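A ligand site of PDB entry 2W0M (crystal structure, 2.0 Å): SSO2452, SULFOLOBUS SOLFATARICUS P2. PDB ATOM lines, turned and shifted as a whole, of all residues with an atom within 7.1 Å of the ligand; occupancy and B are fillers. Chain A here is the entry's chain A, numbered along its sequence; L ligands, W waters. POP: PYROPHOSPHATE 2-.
The backbone NH (N) of Thr 37 lies within hydrogen-bond range of an oxygen (O6) of the ligand (2.8 Å). O4 of the ligand is in hydrogen-bond range of N of Lys 36, at 3.1 Å. An oxygen (O4) of the ligand lies within hydrogen-bond range of the backbone NH (N) of Thr 34. The side-chain hydroxyl of Thr 37 sits at hydrogen-bond distance from an oxygen (O6) of the ligand, at 2.9 Å. An oxygen (O3) of the ligand is in hydrogen-bond range of the backbone NH of Ile 38. N of Gly 33 is in hydrogen-bond range of O5 of the ligand (2.7 Å). An oxygen (O4) of the ligand lies within hydrogen-bond range of the side-chain hydroxyl (OG1) of Thr 34 (3.2 Å). The backbone NH (N) of Gly 35 sits at hydrogen-bond distance from an oxygen (O) of the ligand (3.0 Å). The side-chain amino group of Lys 36 is in salt-bridge range of an oxygen (O4) of the ligand.
Water W1 lies within hydrogen-bond range of an oxygen (O6) of the ligand (2.7 Å), the side-chain carboxylate (OD1) of Asp 130 (2.8 Å), the side-chain amide nitrogen (NE2) of Gln 166 (2.9 Å) and the side-chain hydroxyl (OG1) of Thr 37 (3.1 Å).
Glu 31 touches the ligand. C of Pro 32 touches O5 of the ligand, at 3.7 Å. Hydrophobic or aromatic side chains that line the ligand: Ile 38.
The backbone carbonyl oxygen (O) of Lys 36 is in hydrogen-bond range of the side-chain hydroxyl (OG) of Ser 40. The backbone carbonyl oxygen (O) of Gly 33 lies within hydrogen-bond range of the guanidinium group (NH1) of Arg 200, at 2.9 Å. OG1 of Thr 37 is in hydrogen-bond range of OD2 of Asp 130. NZ of Lys 36 is in hydrogen-bond range of O of Glu 31 (3.1 Å). O of Gly 33 is in hydrogen-bond range of NH1 of Arg 191, at 2.6 Å. The side-chain amino group of Lys 36 sits at hydrogen-bond distance from the backbone carbonyl oxygen of Gly 30, at 2.9 Å. The side-chain hydroxyl (OG1) of Thr 34 lies within hydrogen-bond range of the backbone carbonyl oxygen (O) of Glu 31, 2.6 Å away.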
ATOM      1  N   THR A  29     -17.665 -23.017   5.939  1.00  0.00           N
ATOM      2  CA  THR A  29     -16.578 -22.096   6.139  1.00  0.00           C
ATOM      3  C   THR A  29     -15.267 -22.669   5.596  1.00  0.00           C
ATOM      4  O   THR A  29     -15.072 -23.886   5.526  1.00  0.00           O
ATOM      5  CB  THR A  29     -16.411 -21.782   7.629  1.00  0.00           C
ATOM      6  OG1 THR A  29     -15.975 -22.962   8.305  1.00  0.00           O
ATOM      7  CG2 THR A  29     -17.731 -21.318   8.233  1.00  0.00           C
ATOM      8  N   GLY A  30     -14.371 -21.772   5.203  1.00  0.00           N
ATOM      9  CA  GLY A  30     -13.111 -22.181   4.605  1.00  0.00           C
ATOM     10  C   GLY A  30     -12.593 -21.209   3.584  1.00  0.00           C
ATOM     11  O   GLY A  30     -13.327 -20.403   3.009  1.00  0.00           O
ATOM     12  N   GLU A  31     -11.290 -21.292   3.355  1.00  0.00           N
ATOM     13  CA  GLU A  31     -10.583 -20.480   2.387  1.00  0.00           C
ATOM     14  C   GLU A  31     -11.255 -20.595   1.022  1.00  0.00           C
ATOM     15  O   GLU A  31     -12.013 -21.535   0.764  1.00  0.00           O
ATOM     16  CB  GLU A  31      -9.142 -20.988   2.320  1.00  0.00           C
ATOM     17  CG  GLU A  31      -8.139 -20.067   1.696  1.00  0.00           C
ATOM     18  CD  GLU A  31      -6.793 -20.761   1.533  1.00  0.00           C
ATOM     19  OE1 GLU A  31      -6.746 -21.993   1.734  1.00  0.00           O
ATOM     20  OE2 GLU A  31      -5.789 -20.079   1.211  1.00  0.00           O
ATOM     21  N   PRO A  32     -11.002 -19.625   0.125  1.00  0.00           N
ATOM     22  CA  PRO A  32     -11.478 -19.801  -1.247  1.00  0.00           C
ATOM     23  C   PRO A  32     -10.839 -21.012  -1.916  1.00  0.00           C
ATOM     24  O   PRO A  32      -9.686 -21.329  -1.653  1.00  0.00           O
ATOM     25  CB  PRO A  32     -11.033 -18.509  -1.944  1.00  0.00           C
ATOM     26  CG  PRO A  32     -10.819 -17.528  -0.847  1.00  0.00           C
ATOM     27  CD  PRO A  32     -10.339 -18.319   0.313  1.00  0.00           C
ATOM     28  N   GLY A  33     -11.618 -21.685  -2.757  1.00  0.00           N
ATOM     29  CA  GLY A  33     -11.171 -22.858  -3.512  1.00  0.00           C
ATOM     30  C   GLY A  33     -11.048 -24.133  -2.703  1.00  0.00           C
ATOM     31  O   GLY A  33     -10.202 -24.970  -2.978  1.00  0.00           O
ATOM     32  N   THR A  34     -11.928 -24.305  -1.717  1.00  0.00           N
ATOM     33  CA  THR A  34     -11.848 -25.446  -0.812  1.00  0.00           C
ATOM     34  C   THR A  34     -13.014 -26.422  -0.984  1.00  0.00           C
ATOM     35  O   THR A  34     -13.146 -27.390  -0.239  1.00  0.00           O
ATOM     36  CB  THR A  34     -11.780 -24.989   0.665  1.00  0.00           C
ATOM     37  OG1 THR A  34     -12.767 -23.980   0.906  1.00  0.00           O
ATOM     38  CG2 THR A  34     -10.385 -24.426   0.977  1.00  0.00           C
ATOM     39  N   GLY A  35     -13.864 -26.133  -1.967  1.00  0.00           N
ATOM     40  CA  GLY A  35     -14.931 -27.052  -2.346  1.00  0.00           C
ATOM     41  C   GLY A  35     -16.315 -26.650  -1.863  1.00  0.00           C
ATOM     42  O   GLY A  35     -17.261 -27.415  -2.010  1.00  0.00           O
ATOM     43  N   LYS A  36     -16.439 -25.457  -1.307  1.00  0.00           N
ATOM     44  CA  LYS A  36     -17.707 -25.065  -0.687  1.00  0.00           C
ATOM     45  C   LYS A  36     -18.821 -24.916  -1.725  1.00  0.00           C
ATOM     46  O   LYS A  36     -19.976 -25.282  -1.482  1.00  0.00           O
ATOM     47  CB  LYS A  36     -17.551 -23.762   0.103  1.00  0.00           C
ATOM     48  CG  LYS A  36     -16.493 -23.806   1.208  1.00  0.00           C
ATOM     49  CD  LYS A  36     -16.599 -22.579   2.110  1.00  0.00           C
ATOM     50  CE  LYS A  36     -16.463 -21.285   1.353  1.00  0.00           C
ATOM     51  NZ  LYS A  36     -15.074 -21.046   0.846  1.00  0.00           N
ATOM     52  N   THR A  37     -18.478 -24.359  -2.881  1.00  0.00           N
ATOM     53  CA  THR A  37     -19.490 -24.211  -3.932  1.00  0.00           C
ATOM     54  C   THR A  37     -19.929 -25.592  -4.432  1.00  0.00           C
ATOM     55  O   THR A  37     -21.125 -25.845  -4.546  1.00  0.00           O
ATOM     56  CB  THR A  37     -19.013 -23.325  -5.090  1.00  0.00           C
ATOM     57  OG1 THR A  37     -18.889 -21.971  -4.609  1.00  0.00           O
ATOM     58  CG2 THR A  37     -20.002 -23.379  -6.255  1.00  0.00           C
ATOM     59  N   ILE A  38     -18.984 -26.480  -4.690  1.00  0.00           N
ATOM     60  CA  ILE A  38     -19.316 -27.821  -5.173  1.00  0.00           C
ATOM     61  C   ILE A  38     -20.200 -28.534  -4.161  1.00  0.00           C
ATOM     62  O   ILE A  38     -21.205 -29.138  -4.515  1.00  0.00           O
ATOM     63  CB  ILE A  38     -18.072 -28.691  -5.472  1.00  0.00           C
ATOM     64  CG1 ILE A  38     -17.181 -28.022  -6.507  1.00  0.00           C
ATOM     65  CG2 ILE A  38     -18.480 -30.069  -6.020  1.00  0.00           C
ATOM     66  CD1 ILE A  38     -17.969 -27.287  -7.544  1.00  0.00           C
ATOM     67  N   PHE A  39     -19.838 -28.448  -2.877  1.00  0.00           N
ATOM     68  CA  PHE A  39     -20.622 -29.089  -1.814  1.00  0.00           C
ATOM     69  C   PHE A  39     -22.070 -28.613  -1.879  1.00  0.00           C
ATOM     70  O   PHE A  39     -23.023 -29.391  -1.696  1.00  0.00           O
ATOM     71  CB  PHE A  39     -20.011 -28.768  -0.449  1.00  0.00           C
ATOM     72  CG  PHE A  39     -20.640 -29.520   0.697  1.00  0.00           C
ATOM     73  CD1 PHE A  39     -20.236 -30.814   0.997  1.00  0.00           C
ATOM     74  CD2 PHE A  39     -21.625 -28.950   1.460  1.00  0.00           C
ATOM     75  CE1 PHE A  39     -20.826 -31.506   2.033  1.00  0.00           C
ATOM     76  CE2 PHE A  39     -22.204 -29.644   2.504  1.00  0.00           C
ATOM     77  CZ  PHE A  39     -21.809 -30.916   2.786  1.00  0.00           C
ATOM     78  N   SER A  40     -22.213 -27.333  -2.170  1.00  0.00           N
ATOM     79  CA  SER A  40     -23.513 -26.695  -2.286  1.00  0.00           C
ATOM     80  C   SER A  40     -24.279 -27.145  -3.526  1.00  0.00           C
ATOM     81  O   SER A  40     -25.499 -27.348  -3.478  1.00  0.00           O
ATOM     82  CB  SER A  40     -23.349 -25.177  -2.304  1.00  0.00           C
ATOM     83  OG  SER A  40     -22.822 -24.698  -1.079  1.00  0.00           O
ATOM     84  N   LEU A  41     -23.572 -27.276  -4.653  1.00  0.00           N
ATOM     85  CA  LEU A  41     -24.193 -27.756  -5.876  1.00  0.00           C
ATOM     86  C   LEU A  41     -24.777 -29.151  -5.663  1.00  0.00           C
ATOM     87  O   LEU A  41     -25.820 -29.476  -6.206  1.00  0.00           O
ATOM     88  CB  LEU A  41     -23.204 -27.763  -7.036  1.00  0.00           C
ATOM     89  CG  LEU A  41     -22.747 -26.377  -7.507  1.00  0.00           C
ATOM     90  CD1 LEU A  41     -21.638 -26.489  -8.554  1.00  0.00           C
ATOM     91  CD2 LEU A  41     -23.919 -25.551  -8.039  1.00  0.00           C
ATOM     92  N   TYR A  56     -30.487 -20.841  -5.570  1.00  0.00           N
ATOM     93  CA  TYR A  56     -29.067 -20.634  -5.408  1.00  0.00           C
ATOM     94  C   TYR A  56     -28.766 -19.168  -5.593  1.00  0.00           C
ATOM     95  O   TYR A  56     -28.970 -18.629  -6.691  1.00  0.00           O
ATOM     96  CB  TYR A  56     -28.292 -21.452  -6.426  1.00  0.00           C
ATOM     97  CG  TYR A  56     -26.826 -21.649  -6.060  1.00  0.00           C
ATOM     98  CD1 TYR A  56     -26.354 -22.906  -5.733  1.00  0.00           C
ATOM     99  CD2 TYR A  56     -25.950 -20.574  -6.001  1.00  0.00           C
ATOM    100  CE1 TYR A  56     -25.037 -23.092  -5.382  1.00  0.00           C
ATOM    101  CE2 TYR A  56     -24.635 -20.760  -5.660  1.00  0.00           C
ATOM    102  CZ  TYR A  56     -24.182 -22.024  -5.360  1.00  0.00           C
ATOM    103  OH  TYR A  56     -22.862 -22.221  -4.990  1.00  0.00           O
ATOM    104  N   GLU A  61     -19.722 -15.279  -8.452  1.00  0.00           N
ATOM    105  CA  GLU A  61     -19.728 -15.778  -9.811  1.00  0.00           C
ATOM    106  C   GLU A  61     -21.027 -15.419 -10.500  1.00  0.00           C
ATOM    107  O   GLU A  61     -21.983 -14.940  -9.880  1.00  0.00           O
ATOM    108  CB  GLU A  61     -19.602 -17.297  -9.852  1.00  0.00           C
ATOM    109  CG  GLU A  61     -18.454 -17.867  -9.039  1.00  0.00           C
ATOM    110  CD  GLU A  61     -18.565 -19.374  -8.901  1.00  0.00           C
ATOM    111  OE1 GLU A  61     -19.234 -19.989  -9.767  1.00  0.00           O
ATOM    112  OE2 GLU A  61     -17.999 -19.941  -7.930  1.00  0.00           O
ATOM    113  N   GLN A  69     -20.479 -25.041 -13.929  1.00  0.00           N
ATOM    114  CA  GLN A  69     -19.801 -25.804 -12.888  1.00  0.00           C
ATOM    115  C   GLN A  69     -20.554 -27.091 -12.601  1.00  0.00           C
ATOM    116  O   GLN A  69     -19.955 -28.165 -12.475  1.00  0.00           O
ATOM    117  CB  GLN A  69     -19.691 -24.992 -11.596  1.00  0.00           C
ATOM    118  CG  GLN A  69     -18.506 -24.054 -11.573  1.00  0.00           C
ATOM    119  CD  GLN A  69     -18.164 -23.604 -10.172  1.00  0.00           C
ATOM    120  OE1 GLN A  69     -17.558 -24.348  -9.401  1.00  0.00           O
ATOM    121  NE2 GLN A  69     -18.556 -22.380  -9.839  1.00  0.00           N
ATOM    122  N   ASP A 130     -24.309 -18.140  -1.439  1.00  0.00           N
ATOM    123  CA  ASP A 130     -22.887 -18.301  -1.719  1.00  0.00           C
ATOM    124  C   ASP A 130     -22.345 -16.986  -2.294  1.00  0.00           C
ATOM    125  O   ASP A 130     -22.369 -16.804  -3.507  1.00  0.00           O
ATOM    126  CB  ASP A 130     -22.736 -19.428  -2.742  1.00  0.00           C
ATOM    127  CG  ASP A 130     -21.289 -19.799  -3.034  1.00  0.00           C
ATOM    128  OD1 ASP A 130     -20.383 -19.460  -2.242  1.00  0.00           O
ATOM    129  OD2 ASP A 130     -21.063 -20.462  -4.072  1.00  0.00           O
ATOM    130  N   THR A 164     -22.326 -19.978   2.677  1.00  0.00           N
ATOM    131  CA  THR A 164     -20.878 -20.036   2.630  1.00  0.00           C
ATOM    132  C   THR A 164     -20.288 -18.739   3.132  1.00  0.00           C
ATOM    133  O   THR A 164     -20.882 -17.677   2.994  1.00  0.00           O
ATOM    134  CB  THR A 164     -20.321 -20.297   1.216  1.00  0.00           C
ATOM    135  OG1 THR A 164     -20.439 -19.114   0.423  1.00  0.00           O
ATOM    136  CG2 THR A 164     -21.051 -21.467   0.544  1.00  0.00           C
ATOM    137  N   GLN A 166     -16.182 -16.948   3.309  1.00  0.00           N
ATOM    138  CA  GLN A 166     -14.750 -17.049   3.059  1.00  0.00           C
ATOM    139  C   GLN A 166     -13.987 -16.075   3.954  1.00  0.00           C
ATOM    140  O   GLN A 166     -14.529 -15.053   4.367  1.00  0.00           O
ATOM    141  CB  GLN A 166     -14.409 -16.743   1.599  1.00  0.00           C
ATOM    142  CG  GLN A 166     -14.928 -17.781   0.593  1.00  0.00           C
ATOM    143  CD  GLN A 166     -16.209 -17.344  -0.089  1.00  0.00           C
ATOM    144  OE1 GLN A 166     -16.425 -16.138  -0.312  1.00  0.00           O
ATOM    145  NE2 GLN A 166     -17.075 -18.304  -0.424  1.00  0.00           N
ATOM    146  N   PHE A 189     -14.126 -26.557   5.547  1.00  0.00           N
ATOM    147  CA  PHE A 189     -13.393 -27.063   4.383  1.00  0.00           C
ATOM    148  C   PHE A 189     -11.966 -26.554   4.398  1.00  0.00           C
ATOM    149  O   PHE A 189     -11.727 -25.363   4.590  1.00  0.00           O
ATOM    150  CB  PHE A 189     -14.060 -26.594   3.084  1.00  0.00           C
ATOM    151  CG  PHE A 189     -15.476 -27.047   2.934  1.00  0.00           C
ATOM    152  CD1 PHE A 189     -15.813 -27.978   1.980  1.00  0.00           C
ATOM    153  CD2 PHE A 189     -16.462 -26.557   3.767  1.00  0.00           C
ATOM    154  CE1 PHE A 189     -17.124 -28.402   1.848  1.00  0.00           C
ATOM    155  CE2 PHE A 189     -17.785 -26.978   3.627  1.00  0.00           C
ATOM    156  CZ  PHE A 189     -18.098 -27.894   2.668  1.00  0.00           C
ATOM    157  N   ARG A 191      -7.831 -26.898   2.555  1.00  0.00           N
ATOM    158  CA  ARG A 191      -6.915 -27.399   1.532  1.00  0.00           C
ATOM    159  C   ARG A 191      -5.483 -27.197   2.010  1.00  0.00           C
ATOM    160  O   ARG A 191      -5.171 -26.246   2.713  1.00  0.00           O
ATOM    161  CB  ARG A 191      -7.136 -26.708   0.185  1.00  0.00           C
ATOM    162  CG  ARG A 191      -6.965 -25.200   0.206  1.00  0.00           C
ATOM    163  CD  ARG A 191      -7.282 -24.601  -1.151  1.00  0.00           C
ATOM    164  NE  ARG A 191      -6.328 -25.038  -2.161  1.00  0.00           N
ATOM    165  CZ  ARG A 191      -6.598 -25.163  -3.467  1.00  0.00           C
ATOM    166  NH1 ARG A 191      -7.818 -24.897  -3.921  1.00  0.00           N
ATOM    167  NH2 ARG A 191      -5.644 -25.555  -4.301  1.00  0.00           N
ATOM    168  N   ARG A 200      -7.408 -32.136   0.315  1.00  0.00           N
ATOM    169  CA  ARG A 200      -8.586 -31.419   0.758  1.00  0.00           C
ATOM    170  C   ARG A 200      -9.255 -32.184   1.882  1.00  0.00           C
ATOM    171  O   ARG A 200      -9.322 -33.407   1.865  1.00  0.00           O
ATOM    172  CB  ARG A 200      -9.589 -31.265  -0.388  1.00  0.00           C
ATOM    173  CG  ARG A 200      -9.079 -30.529  -1.578  1.00  0.00           C
ATOM    174  CD  ARG A 200     -10.085 -30.619  -2.699  1.00  0.00           C
ATOM    175  NE  ARG A 200      -9.652 -29.898  -3.892  1.00  0.00           N
ATOM    176  CZ  ARG A 200      -9.785 -28.586  -4.040  1.00  0.00           C
ATOM    177  NH1 ARG A 200     -10.333 -27.878  -3.068  1.00  0.00           N
ATOM    178  NH2 ARG A 200      -9.370 -27.992  -5.150  1.00  0.00           N
ATOM    179  N   ILE A 221     -12.253 -33.963  -5.290  1.00  0.00           N
ATOM    180  CA  ILE A 221     -13.200 -33.417  -6.253  1.00  0.00           C
ATOM    181  C   ILE A 221     -12.900 -34.062  -7.607  1.00  0.00           C
ATOM    182  O   ILE A 221     -11.864 -33.801  -8.205  1.00  0.00           O
ATOM    183  CB  ILE A 221     -13.107 -31.876  -6.367  1.00  0.00           C
ATOM    184  CG1 ILE A 221     -13.287 -31.236  -4.990  1.00  0.00           C
ATOM    185  CG2 ILE A 221     -14.155 -31.351  -7.337  1.00  0.00           C
ATOM    186  CD1 ILE A 221     -13.269 -29.707  -5.014  1.00  0.00           C
ATOM    187  N   ILE A 227     -17.673 -34.111  -5.099  1.00  0.00           N
ATOM    188  CA  ILE A 227     -16.933 -34.403  -3.874  1.00  0.00           C
ATOM    189  C   ILE A 227     -17.014 -35.880  -3.505  1.00  0.00           C
ATOM    190  O   ILE A 227     -18.098 -36.448  -3.398  1.00  0.00           O
ATOM    191  CB  ILE A 227     -17.446 -33.574  -2.691  1.00  0.00           C
ATOM    192  CG1 ILE A 227     -17.086 -32.101  -2.900  1.00  0.00           C
ATOM    193  CG2 ILE A 227     -16.858 -34.067  -1.395  1.00  0.00           C
ATOM    194  CD1 ILE A 227     -17.788 -31.188  -1.969  1.00  0.00           C
HETATM  195  P1  POP L   1     -15.201 -24.347  -5.024  1.00  0.00           P
HETATM  196  O1  POP L   1     -14.235 -24.918  -6.040  1.00  0.00           O
HETATM  197  O2  POP L   1     -15.863 -23.128  -5.625  1.00  0.00           O
HETATM  198  O3  POP L   1     -16.251 -25.355  -4.649  1.00  0.00           O
HETATM  199  O   POP L   1     -14.324 -23.828  -3.778  1.00  0.00           O
HETATM  200  P2  POP L   1     -14.914 -22.593  -2.926  1.00  0.00           P
HETATM  201  O4  POP L   1     -14.689 -22.904  -1.466  1.00  0.00           O
HETATM  202  O5  POP L   1     -14.217 -21.295  -3.282  1.00  0.00           O
HETATM  203  O6  POP L   1     -16.385 -22.455  -3.221  1.00  0.00           O
HETATM  204  O   HOH W   1     -17.868 -20.584  -1.975  1.00  0.00           O
